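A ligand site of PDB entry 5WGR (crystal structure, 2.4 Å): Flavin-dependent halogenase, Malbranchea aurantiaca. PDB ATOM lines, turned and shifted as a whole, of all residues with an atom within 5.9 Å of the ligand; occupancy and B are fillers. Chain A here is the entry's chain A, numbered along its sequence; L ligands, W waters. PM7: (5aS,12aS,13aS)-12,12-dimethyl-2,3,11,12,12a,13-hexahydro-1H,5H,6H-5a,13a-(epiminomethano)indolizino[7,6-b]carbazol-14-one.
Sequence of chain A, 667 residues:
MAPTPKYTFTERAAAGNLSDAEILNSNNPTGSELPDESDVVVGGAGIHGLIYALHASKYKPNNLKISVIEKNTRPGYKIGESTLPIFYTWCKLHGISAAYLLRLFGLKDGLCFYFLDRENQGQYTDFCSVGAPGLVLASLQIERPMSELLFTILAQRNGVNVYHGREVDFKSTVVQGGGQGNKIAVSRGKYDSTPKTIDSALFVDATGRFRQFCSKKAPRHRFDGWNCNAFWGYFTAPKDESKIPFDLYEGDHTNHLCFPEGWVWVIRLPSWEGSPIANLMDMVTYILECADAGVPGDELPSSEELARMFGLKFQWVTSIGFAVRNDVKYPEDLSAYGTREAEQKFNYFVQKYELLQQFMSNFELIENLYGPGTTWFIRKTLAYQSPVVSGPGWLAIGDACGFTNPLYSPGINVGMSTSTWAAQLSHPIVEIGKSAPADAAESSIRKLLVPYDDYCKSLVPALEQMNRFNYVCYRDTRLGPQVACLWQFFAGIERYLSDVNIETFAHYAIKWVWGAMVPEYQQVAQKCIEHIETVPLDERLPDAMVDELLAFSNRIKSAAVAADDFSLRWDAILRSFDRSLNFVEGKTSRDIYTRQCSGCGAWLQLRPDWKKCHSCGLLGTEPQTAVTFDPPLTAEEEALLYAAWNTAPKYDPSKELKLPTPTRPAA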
ATOM      1  N   PRO A  85      -9.055 -23.261 -20.205  1.00  0.00           N
ATOM      2  CA  PRO A  85      -8.779 -21.820 -20.038  1.00  0.00           C
ATOM      3  C   PRO A  85      -7.367 -21.478 -19.611  1.00  0.00           C
ATOM      4  O   PRO A  85      -6.823 -20.481 -20.096  1.00  0.00           O
ATOM      5  CB  PRO A  85      -9.802 -21.415 -18.962  1.00  0.00           C
ATOM      6  CG  PRO A  85     -10.963 -22.338 -19.200  1.00  0.00           C
ATOM      7  CD  PRO A  85     -10.383 -23.642 -19.658  1.00  0.00           C
ATOM      8  N   LEU A 111     -17.482 -28.332 -21.277  1.00  0.00           N
ATOM      9  CA  LEU A 111     -17.430 -29.775 -21.235  1.00  0.00           C
ATOM     10  C   LEU A 111     -18.846 -30.300 -20.983  1.00  0.00           C
ATOM     11  O   LEU A 111     -19.557 -29.783 -20.115  1.00  0.00           O
ATOM     12  CB  LEU A 111     -16.488 -30.267 -20.128  1.00  0.00           C
ATOM     13  CG  LEU A 111     -14.971 -30.003 -20.197  1.00  0.00           C
ATOM     14  CD1 LEU A 111     -14.603 -28.541 -19.895  1.00  0.00           C
ATOM     15  CD2 LEU A 111     -14.255 -30.937 -19.219  1.00  0.00           C
ATOM     16  N   SER A 129     -21.905 -27.940 -19.111  1.00  0.00           N
ATOM     17  CA  SER A 129     -21.336 -26.668 -18.674  1.00  0.00           C
ATOM     18  C   SER A 129     -21.057 -25.819 -19.905  1.00  0.00           C
ATOM     19  O   SER A 129     -21.257 -26.252 -21.052  1.00  0.00           O
ATOM     20  CB  SER A 129     -20.049 -26.866 -17.851  1.00  0.00           C
ATOM     21  OG  SER A 129     -18.979 -27.276 -18.675  1.00  0.00           O
ATOM     22  N   VAL A 130     -20.603 -24.588 -19.683  1.00  0.00           N
ATOM     23  CA  VAL A 130     -20.335 -23.658 -20.763  1.00  0.00           C
ATOM     24  C   VAL A 130     -18.904 -23.158 -20.642  1.00  0.00           C
ATOM     25  O   VAL A 130     -18.237 -23.333 -19.615  1.00  0.00           O
ATOM     26  CB  VAL A 130     -21.313 -22.472 -20.751  1.00  0.00           C
ATOM     27  CG1 VAL A 130     -22.747 -22.969 -20.923  1.00  0.00           C
ATOM     28  CG2 VAL A 130     -21.153 -21.697 -19.450  1.00  0.00           C
ATOM     29  N   GLY A 131     -18.425 -22.548 -21.726  1.00  0.00           N
ATOM     30  CA  GLY A 131     -17.158 -21.846 -21.721  1.00  0.00           C
ATOM     31  C   GLY A 131     -17.314 -20.414 -21.225  1.00  0.00           C
ATOM     32  O   GLY A 131     -17.662 -20.193 -20.075  1.00  0.00           O
ATOM     33  N   ALA A 132     -17.078 -19.437 -22.100  1.00  0.00           N
ATOM     34  CA  ALA A 132     -17.076 -18.043 -21.689  1.00  0.00           C
ATOM     35  C   ALA A 132     -17.462 -17.184 -22.880  1.00  0.00           C
ATOM     36  O   ALA A 132     -17.363 -17.638 -24.029  1.00  0.00           O
ATOM     37  CB  ALA A 132     -15.695 -17.629 -21.141  1.00  0.00           C
ATOM     38  N   PRO A 133     -17.916 -15.953 -22.651  1.00  0.00           N
ATOM     39  CA  PRO A 133     -18.185 -15.055 -23.775  1.00  0.00           C
ATOM     40  C   PRO A 133     -16.935 -14.827 -24.612  1.00  0.00           C
ATOM     41  O   PRO A 133     -15.804 -14.880 -24.118  1.00  0.00           O
ATOM     42  CB  PRO A 133     -18.644 -13.754 -23.101  1.00  0.00           C
ATOM     43  CG  PRO A 133     -19.207 -14.196 -21.792  1.00  0.00           C
ATOM     44  CD  PRO A 133     -18.392 -15.385 -21.367  1.00  0.00           C
ATOM     45  N   VAL A 136     -14.404 -12.692 -23.194  1.00  0.00           N
ATOM     46  CA  VAL A 136     -13.722 -13.096 -21.969  1.00  0.00           C
ATOM     47  C   VAL A 136     -12.507 -13.950 -22.334  1.00  0.00           C
ATOM     48  O   VAL A 136     -11.360 -13.514 -22.193  1.00  0.00           O
ATOM     49  CB  VAL A 136     -14.682 -13.826 -21.027  1.00  0.00           C
ATOM     50  CG1 VAL A 136     -13.966 -14.281 -19.770  1.00  0.00           C
ATOM     51  CG2 VAL A 136     -15.844 -12.905 -20.653  1.00  0.00           C
ATOM     52  N   LEU A 137     -12.746 -15.171 -22.809  1.00  0.00           N
ATOM     53  CA  LEU A 137     -11.666 -16.044 -23.274  1.00  0.00           C
ATOM     54  C   LEU A 137     -12.263 -17.127 -24.167  1.00  0.00           C
ATOM     55  O   LEU A 137     -13.466 -17.155 -24.428  1.00  0.00           O
ATOM     56  CB  LEU A 137     -10.885 -16.642 -22.098  1.00  0.00           C
ATOM     57  CG  LEU A 137     -11.620 -17.412 -21.002  1.00  0.00           C
ATOM     58  CD1 LEU A 137     -11.948 -18.849 -21.435  1.00  0.00           C
ATOM     59  CD2 LEU A 137     -10.809 -17.422 -19.713  1.00  0.00           C
ATOM     60  N   PHE A 489     -15.880 -29.613 -11.028  1.00  0.00           N
ATOM     61  CA  PHE A 489     -16.046 -28.230 -11.461  1.00  0.00           C
ATOM     62  C   PHE A 489     -16.033 -27.269 -10.281  1.00  0.00           C
ATOM     63  O   PHE A 489     -15.542 -26.143 -10.408  1.00  0.00           O
ATOM     64  CB  PHE A 489     -17.335 -28.087 -12.264  1.00  0.00           C
ATOM     65  CG  PHE A 489     -17.272 -28.703 -13.626  1.00  0.00           C
ATOM     66  CD1 PHE A 489     -17.106 -30.071 -13.776  1.00  0.00           C
ATOM     67  CD2 PHE A 489     -17.391 -27.934 -14.752  1.00  0.00           C
ATOM     68  CE1 PHE A 489     -17.050 -30.639 -15.030  1.00  0.00           C
ATOM     69  CE2 PHE A 489     -17.334 -28.502 -16.005  1.00  0.00           C
ATOM     70  CZ  PHE A 489     -17.164 -29.855 -16.144  1.00  0.00           C
ATOM     71  N   GLY A 492     -12.308 -27.354  -9.068  1.00  0.00           N
ATOM     72  CA  GLY A 492     -11.293 -27.078 -10.063  1.00  0.00           C
ATOM     73  C   GLY A 492     -11.530 -25.888 -10.969  1.00  0.00           C
ATOM     74  O   GLY A 492     -10.755 -25.655 -11.908  1.00  0.00           O
ATOM     75  N   ILE A 493     -12.593 -25.128 -10.736  1.00  0.00           N
ATOM     76  CA  ILE A 493     -12.815 -23.937 -11.550  1.00  0.00           C
ATOM     77  C   ILE A 493     -11.748 -22.887 -11.215  1.00  0.00           C
ATOM     78  O   ILE A 493     -11.330 -22.752 -10.054  1.00  0.00           O
ATOM     79  CB  ILE A 493     -14.246 -23.404 -11.371  1.00  0.00           C
ATOM     80  CG1 ILE A 493     -14.555 -22.336 -12.409  1.00  0.00           C
ATOM     81  CG2 ILE A 493     -14.486 -22.942  -9.940  1.00  0.00           C
ATOM     82  CD1 ILE A 493     -16.034 -22.098 -12.621  1.00  0.00           C
ATOM     83  N   GLU A 494     -11.282 -22.176 -12.237  1.00  0.00           N
ATOM     84  CA  GLU A 494     -10.035 -21.399 -12.152  1.00  0.00           C
ATOM     85  C   GLU A 494     -10.317 -20.013 -11.594  1.00  0.00           C
ATOM     86  O   GLU A 494     -10.315 -19.004 -12.309  1.00  0.00           O
ATOM     87  CB  GLU A 494      -9.367 -21.330 -13.519  1.00  0.00           C
ATOM     88  CG  GLU A 494      -9.076 -22.684 -14.171  1.00  0.00           C
ATOM     89  CD  GLU A 494     -10.155 -23.118 -15.172  1.00  0.00           C
ATOM     90  OE1 GLU A 494     -11.343 -22.778 -14.973  1.00  0.00           O
ATOM     91  OE2 GLU A 494      -9.799 -23.787 -16.163  1.00  0.00           O
ATOM     92  N   ARG A 495     -10.548 -19.958 -10.287  1.00  0.00           N
ATOM     93  CA  ARG A 495     -10.802 -18.684  -9.617  1.00  0.00           C
ATOM     94  C   ARG A 495      -9.608 -17.747  -9.758  1.00  0.00           C
ATOM     95  O   ARG A 495      -8.464 -18.152  -9.593  1.00  0.00           O
ATOM     96  CB  ARG A 495     -11.125 -18.923  -8.135  1.00  0.00           C
ATOM     97  CG  ARG A 495     -12.367 -19.794  -7.890  1.00  0.00           C
ATOM     98  CD  ARG A 495     -12.489 -20.181  -6.408  1.00  0.00           C
ATOM     99  NE  ARG A 495     -13.674 -20.983  -6.140  1.00  0.00           N
ATOM    100  CZ  ARG A 495     -13.773 -22.282  -6.413  1.00  0.00           C
ATOM    101  NH1 ARG A 495     -12.736 -22.923  -6.951  1.00  0.00           N
ATOM    102  NH2 ARG A 495     -14.902 -22.934  -6.159  1.00  0.00           N
ATOM    103  N   LEU A 497      -8.316 -16.357 -12.382  1.00  0.00           N
ATOM    104  CA  LEU A 497      -7.469 -16.548 -13.550  1.00  0.00           C
ATOM    105  C   LEU A 497      -7.226 -15.235 -14.285  1.00  0.00           C
ATOM    106  O   LEU A 497      -6.178 -15.059 -14.921  1.00  0.00           O
ATOM    107  CB  LEU A 497      -8.095 -17.583 -14.491  1.00  0.00           C
ATOM    108  CG  LEU A 497      -7.508 -17.865 -15.881  1.00  0.00           C
ATOM    109  CD1 LEU A 497      -6.152 -18.532 -15.777  1.00  0.00           C
ATOM    110  CD2 LEU A 497      -8.483 -18.745 -16.683  1.00  0.00           C
ATOM    111  N   TRP A 514      -6.582 -29.031 -11.080  1.00  0.00           N
ATOM    112  CA  TRP A 514      -7.989 -29.324 -11.321  1.00  0.00           C
ATOM    113  C   TRP A 514      -8.779 -29.488 -10.015  1.00  0.00           C
ATOM    114  O   TRP A 514      -9.819 -30.167  -9.997  1.00  0.00           O
ATOM    115  CB  TRP A 514      -8.153 -30.587 -12.190  1.00  0.00           C
ATOM    116  CG  TRP A 514      -8.681 -30.344 -13.579  1.00  0.00           C
ATOM    117  CD1 TRP A 514      -8.043 -30.622 -14.747  1.00  0.00           C
ATOM    118  CD2 TRP A 514      -9.962 -29.796 -13.930  1.00  0.00           C
ATOM    119  NE1 TRP A 514      -8.836 -30.276 -15.818  1.00  0.00           N
ATOM    120  CE2 TRP A 514     -10.020 -29.763 -15.339  1.00  0.00           C
ATOM    121  CE3 TRP A 514     -11.051 -29.316 -13.203  1.00  0.00           C
ATOM    122  CZ2 TRP A 514     -11.132 -29.276 -16.036  1.00  0.00           C
ATOM    123  CZ3 TRP A 514     -12.161 -28.835 -13.892  1.00  0.00           C
ATOM    124  CH2 TRP A 514     -12.189 -28.812 -15.302  1.00  0.00           C
ATOM    125  N   LEU A 568     -19.802 -16.444  -8.299  1.00  0.00           N
ATOM    126  CA  LEU A 568     -19.974 -17.068  -9.600  1.00  0.00           C
ATOM    127  C   LEU A 568     -21.461 -17.250  -9.879  1.00  0.00           C
ATOM    128  O   LEU A 568     -22.212 -17.671  -8.998  1.00  0.00           O
ATOM    129  CB  LEU A 568     -19.283 -18.432  -9.664  1.00  0.00           C
ATOM    130  CG  LEU A 568     -17.852 -18.434 -10.159  1.00  0.00           C
ATOM    131  CD1 LEU A 568     -17.227 -19.769  -9.867  1.00  0.00           C
ATOM    132  CD2 LEU A 568     -17.817 -18.141 -11.652  1.00  0.00           C
ATOM    133  N   ILE A 573     -23.754 -21.291 -15.479  1.00  0.00           N
ATOM    134  CA  ILE A 573     -22.553 -21.951 -15.981  1.00  0.00           C
ATOM    135  C   ILE A 573     -22.753 -23.459 -16.031  1.00  0.00           C
ATOM    136  O   ILE A 573     -22.223 -24.139 -16.916  1.00  0.00           O
ATOM    137  CB  ILE A 573     -21.345 -21.577 -15.093  1.00  0.00           C
ATOM    138  CG1 ILE A 573     -21.031 -20.089 -15.265  1.00  0.00           C
ATOM    139  CG2 ILE A 573     -20.119 -22.407 -15.426  1.00  0.00           C
ATOM    140  CD1 ILE A 573     -20.042 -19.567 -14.253  1.00  0.00           C
ATOM    141  N   LEU A 574     -23.520 -23.999 -15.078  1.00  0.00           N
ATOM    142  CA  LEU A 574     -23.884 -25.411 -15.045  1.00  0.00           C
ATOM    143  C   LEU A 574     -25.371 -25.535 -15.313  1.00  0.00           C
ATOM    144  O   LEU A 574     -26.193 -25.004 -14.548  1.00  0.00           O
ATOM    145  CB  LEU A 574     -23.539 -26.041 -13.691  1.00  0.00           C
ATOM    146  CG  LEU A 574     -22.091 -25.914 -13.228  1.00  0.00           C
ATOM    147  CD1 LEU A 574     -21.862 -26.758 -11.972  1.00  0.00           C
ATOM    148  CD2 LEU A 574     -21.114 -26.295 -14.329  1.00  0.00           C
ATOM    149  N   TYR A 593     -22.997 -18.673 -25.378  1.00  0.00           N
ATOM    150  CA  TYR A 593     -21.824 -17.930 -25.814  1.00  0.00           C
ATOM    151  C   TYR A 593     -21.420 -18.230 -27.254  1.00  0.00           C
ATOM    152  O   TYR A 593     -20.551 -17.527 -27.793  1.00  0.00           O
ATOM    153  CB  TYR A 593     -20.618 -18.263 -24.920  1.00  0.00           C
ATOM    154  CG  TYR A 593     -20.817 -18.000 -23.440  1.00  0.00           C
ATOM    155  CD1 TYR A 593     -21.504 -16.886 -22.981  1.00  0.00           C
ATOM    156  CD2 TYR A 593     -20.306 -18.897 -22.503  1.00  0.00           C
ATOM    157  CE1 TYR A 593     -21.666 -16.646 -21.620  1.00  0.00           C
ATOM    158  CE2 TYR A 593     -20.463 -18.680 -21.149  1.00  0.00           C
ATOM    159  CZ  TYR A 593     -21.142 -17.555 -20.708  1.00  0.00           C
ATOM    160  OH  TYR A 593     -21.290 -17.353 -19.355  1.00  0.00           O
ATOM    161  N   LEU A 641     -17.793  -7.157 -16.714  1.00  0.00           N
ATOM    162  CA  LEU A 641     -17.237  -8.488 -16.979  1.00  0.00           C
ATOM    163  C   LEU A 641     -16.123  -8.411 -18.016  1.00  0.00           C
ATOM    164  O   LEU A 641     -14.984  -8.826 -17.753  1.00  0.00           O
ATOM    165  CB  LEU A 641     -18.350  -9.420 -17.458  1.00  0.00           C
ATOM    166  CG  LEU A 641     -18.303 -10.944 -17.246  1.00  0.00           C
ATOM    167  CD1 LEU A 641     -19.181 -11.636 -18.275  1.00  0.00           C
ATOM    168  CD2 LEU A 641     -16.908 -11.542 -17.261  1.00  0.00           C
ATOM    169  N   TRP A 645     -11.295  -8.832 -18.231  1.00  0.00           N
ATOM    170  CA  TRP A 645     -10.589  -9.839 -19.014  1.00  0.00           C
ATOM    171  C   TRP A 645      -9.870  -9.273 -20.229  1.00  0.00           C
ATOM    172  O   TRP A 645      -9.367 -10.045 -21.054  1.00  0.00           O
ATOM    173  CB  TRP A 645     -11.574 -10.909 -19.459  1.00  0.00           C
ATOM    174  CG  TRP A 645     -12.007 -11.792 -18.351  1.00  0.00           C
ATOM    175  CD1 TRP A 645     -13.107 -11.639 -17.558  1.00  0.00           C
ATOM    176  CD2 TRP A 645     -11.339 -12.964 -17.901  1.00  0.00           C
ATOM    177  NE1 TRP A 645     -13.169 -12.656 -16.640  1.00  0.00           N
ATOM    178  CE2 TRP A 645     -12.094 -13.493 -16.833  1.00  0.00           C
ATOM    179  CE3 TRP A 645     -10.174 -13.644 -18.295  1.00  0.00           C
ATOM    180  CZ2 TRP A 645     -11.727 -14.654 -16.151  1.00  0.00           C
ATOM    181  CZ3 TRP A 645      -9.808 -14.799 -17.620  1.00  0.00           C
ATOM    182  CH2 TRP A 645     -10.580 -15.291 -16.558  1.00  0.00           C
HETATM  183  N   PM7 L   1     -17.053 -18.249 -17.927  1.00  0.00           N
HETATM  184  C   PM7 L   1     -16.812 -16.940 -17.828  1.00  0.00           C
HETATM  185  O   PM7 L   1     -17.294 -16.112 -18.591  1.00  0.00           O
HETATM  186  C1  PM7 L   1     -15.860 -16.593 -16.681  1.00  0.00           C
HETATM  187  C10 PM7 L   1     -15.378 -25.520 -15.583  1.00  0.00           C
HETATM  188  C11 PM7 L   1     -14.331 -24.622 -15.481  1.00  0.00           C
HETATM  189  C12 PM7 L   1     -14.553 -23.317 -15.891  1.00  0.00           C
HETATM  190  C13 PM7 L   1     -14.387 -21.142 -16.379  1.00  0.00           C
HETATM  191  C14 PM7 L   1     -13.802 -19.757 -16.472  1.00  0.00           C
HETATM  192  C15 PM7 L   1     -13.451 -19.329 -15.036  1.00  0.00           C
HETATM  193  C16 PM7 L   1     -12.496 -19.830 -17.271  1.00  0.00           C
HETATM  194  C17 PM7 L   1     -16.800 -18.590 -15.553  1.00  0.00           C
HETATM  195  C18 PM7 L   1     -17.535 -16.238 -15.180  1.00  0.00           C
HETATM  196  C19 PM7 L   1     -16.923 -14.855 -15.398  1.00  0.00           C
HETATM  197  C2  PM7 L   1     -14.533 -17.312 -16.963  1.00  0.00           C
HETATM  198  C20 PM7 L   1     -15.779 -15.083 -16.383  1.00  0.00           C
HETATM  199  C3  PM7 L   1     -14.836 -18.806 -17.169  1.00  0.00           C
HETATM  200  C4  PM7 L   1     -16.363 -19.094 -16.934  1.00  0.00           C
HETATM  201  C5  PM7 L   1     -16.684 -20.555 -17.256  1.00  0.00           C
HETATM  202  C6  PM7 L   1     -15.666 -21.498 -16.695  1.00  0.00           C
HETATM  203  C7  PM7 L   1     -15.793 -22.888 -16.378  1.00  0.00           C
HETATM  204  C8  PM7 L   1     -16.829 -23.814 -16.467  1.00  0.00           C
HETATM  205  C9  PM7 L   1     -16.620 -25.119 -16.067  1.00  0.00           C
HETATM  206  N1  PM7 L   1     -13.693 -22.235 -15.905  1.00  0.00           N
HETATM  207  N2  PM7 L   1     -16.439 -17.170 -15.446  1.00  0.00           N
HETATM  208  O   HOH W   1     -14.789 -16.495 -13.498  1.00  0.00           O
HETATM  209  O   HOH W   2     -12.165 -25.352 -17.386  1.00  0.00           O
HETATM  210  O   HOH W   3     -14.595 -21.873 -19.519  1.00  0.00           O
HETATM  211  O   HOH W   4     -16.201 -25.210 -19.149  1.00  0.00           O
HETATM  212  O   HOH W   5     -20.509 -14.608 -15.183  1.00  0.00           O
HETATM  213  O   HOH W   6     -20.013 -15.301 -18.209  1.00  0.00           O
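N of Val 130 lies within hydrogen-bond range of O of Ile 573 (3.2 Å). O of Ile 493 is in hydrogen-bond range of NH1 of Arg 495 (3.4 Å).
The side-chain carboxylate of Glu 494 sits at hydrogen-bond distance from a nitrogen (N1) of the ligand (2.6 Å). The backbone carbonyl oxygen of Gly 131 is in hydrogen-bond range of a nitrogen (N) of the ligand (3.0 Å).
Water W6 bridges the side-chain hydroxyl (OH) of Tyr 593 and an oxygen (O) of the ligand. Water W4 bridges O of Val 130 (2.8 Å) and OG of Ser 129 (3.5 Å).
Merely in contact with the ligand: Pro 85, Val 130, Ala 132, Pro 133, Val 136, Leu 137, Phe 489, Ile 493, Ile 573, Leu 641 and Trp 645. Hydrophobic or aromatic side chains that line the ligand: Pro 85, Ala 132, Pro 133, Val 136, Leu 137, Phe 489, Ile 493, Ile 573, Leu 641 and Trp 645. 13 residues have an atom within 4 Å of the ligand: Pro 85, Val 130, Gly 131, Ala 132, Pro 133, Val 136, Leu 137, Phe 489, Ile 493, Glu 494, Ile 573, Leu 641 and Trp 645. Along chain A the residues within 4 Å of the ligand span positions 85 to 645.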
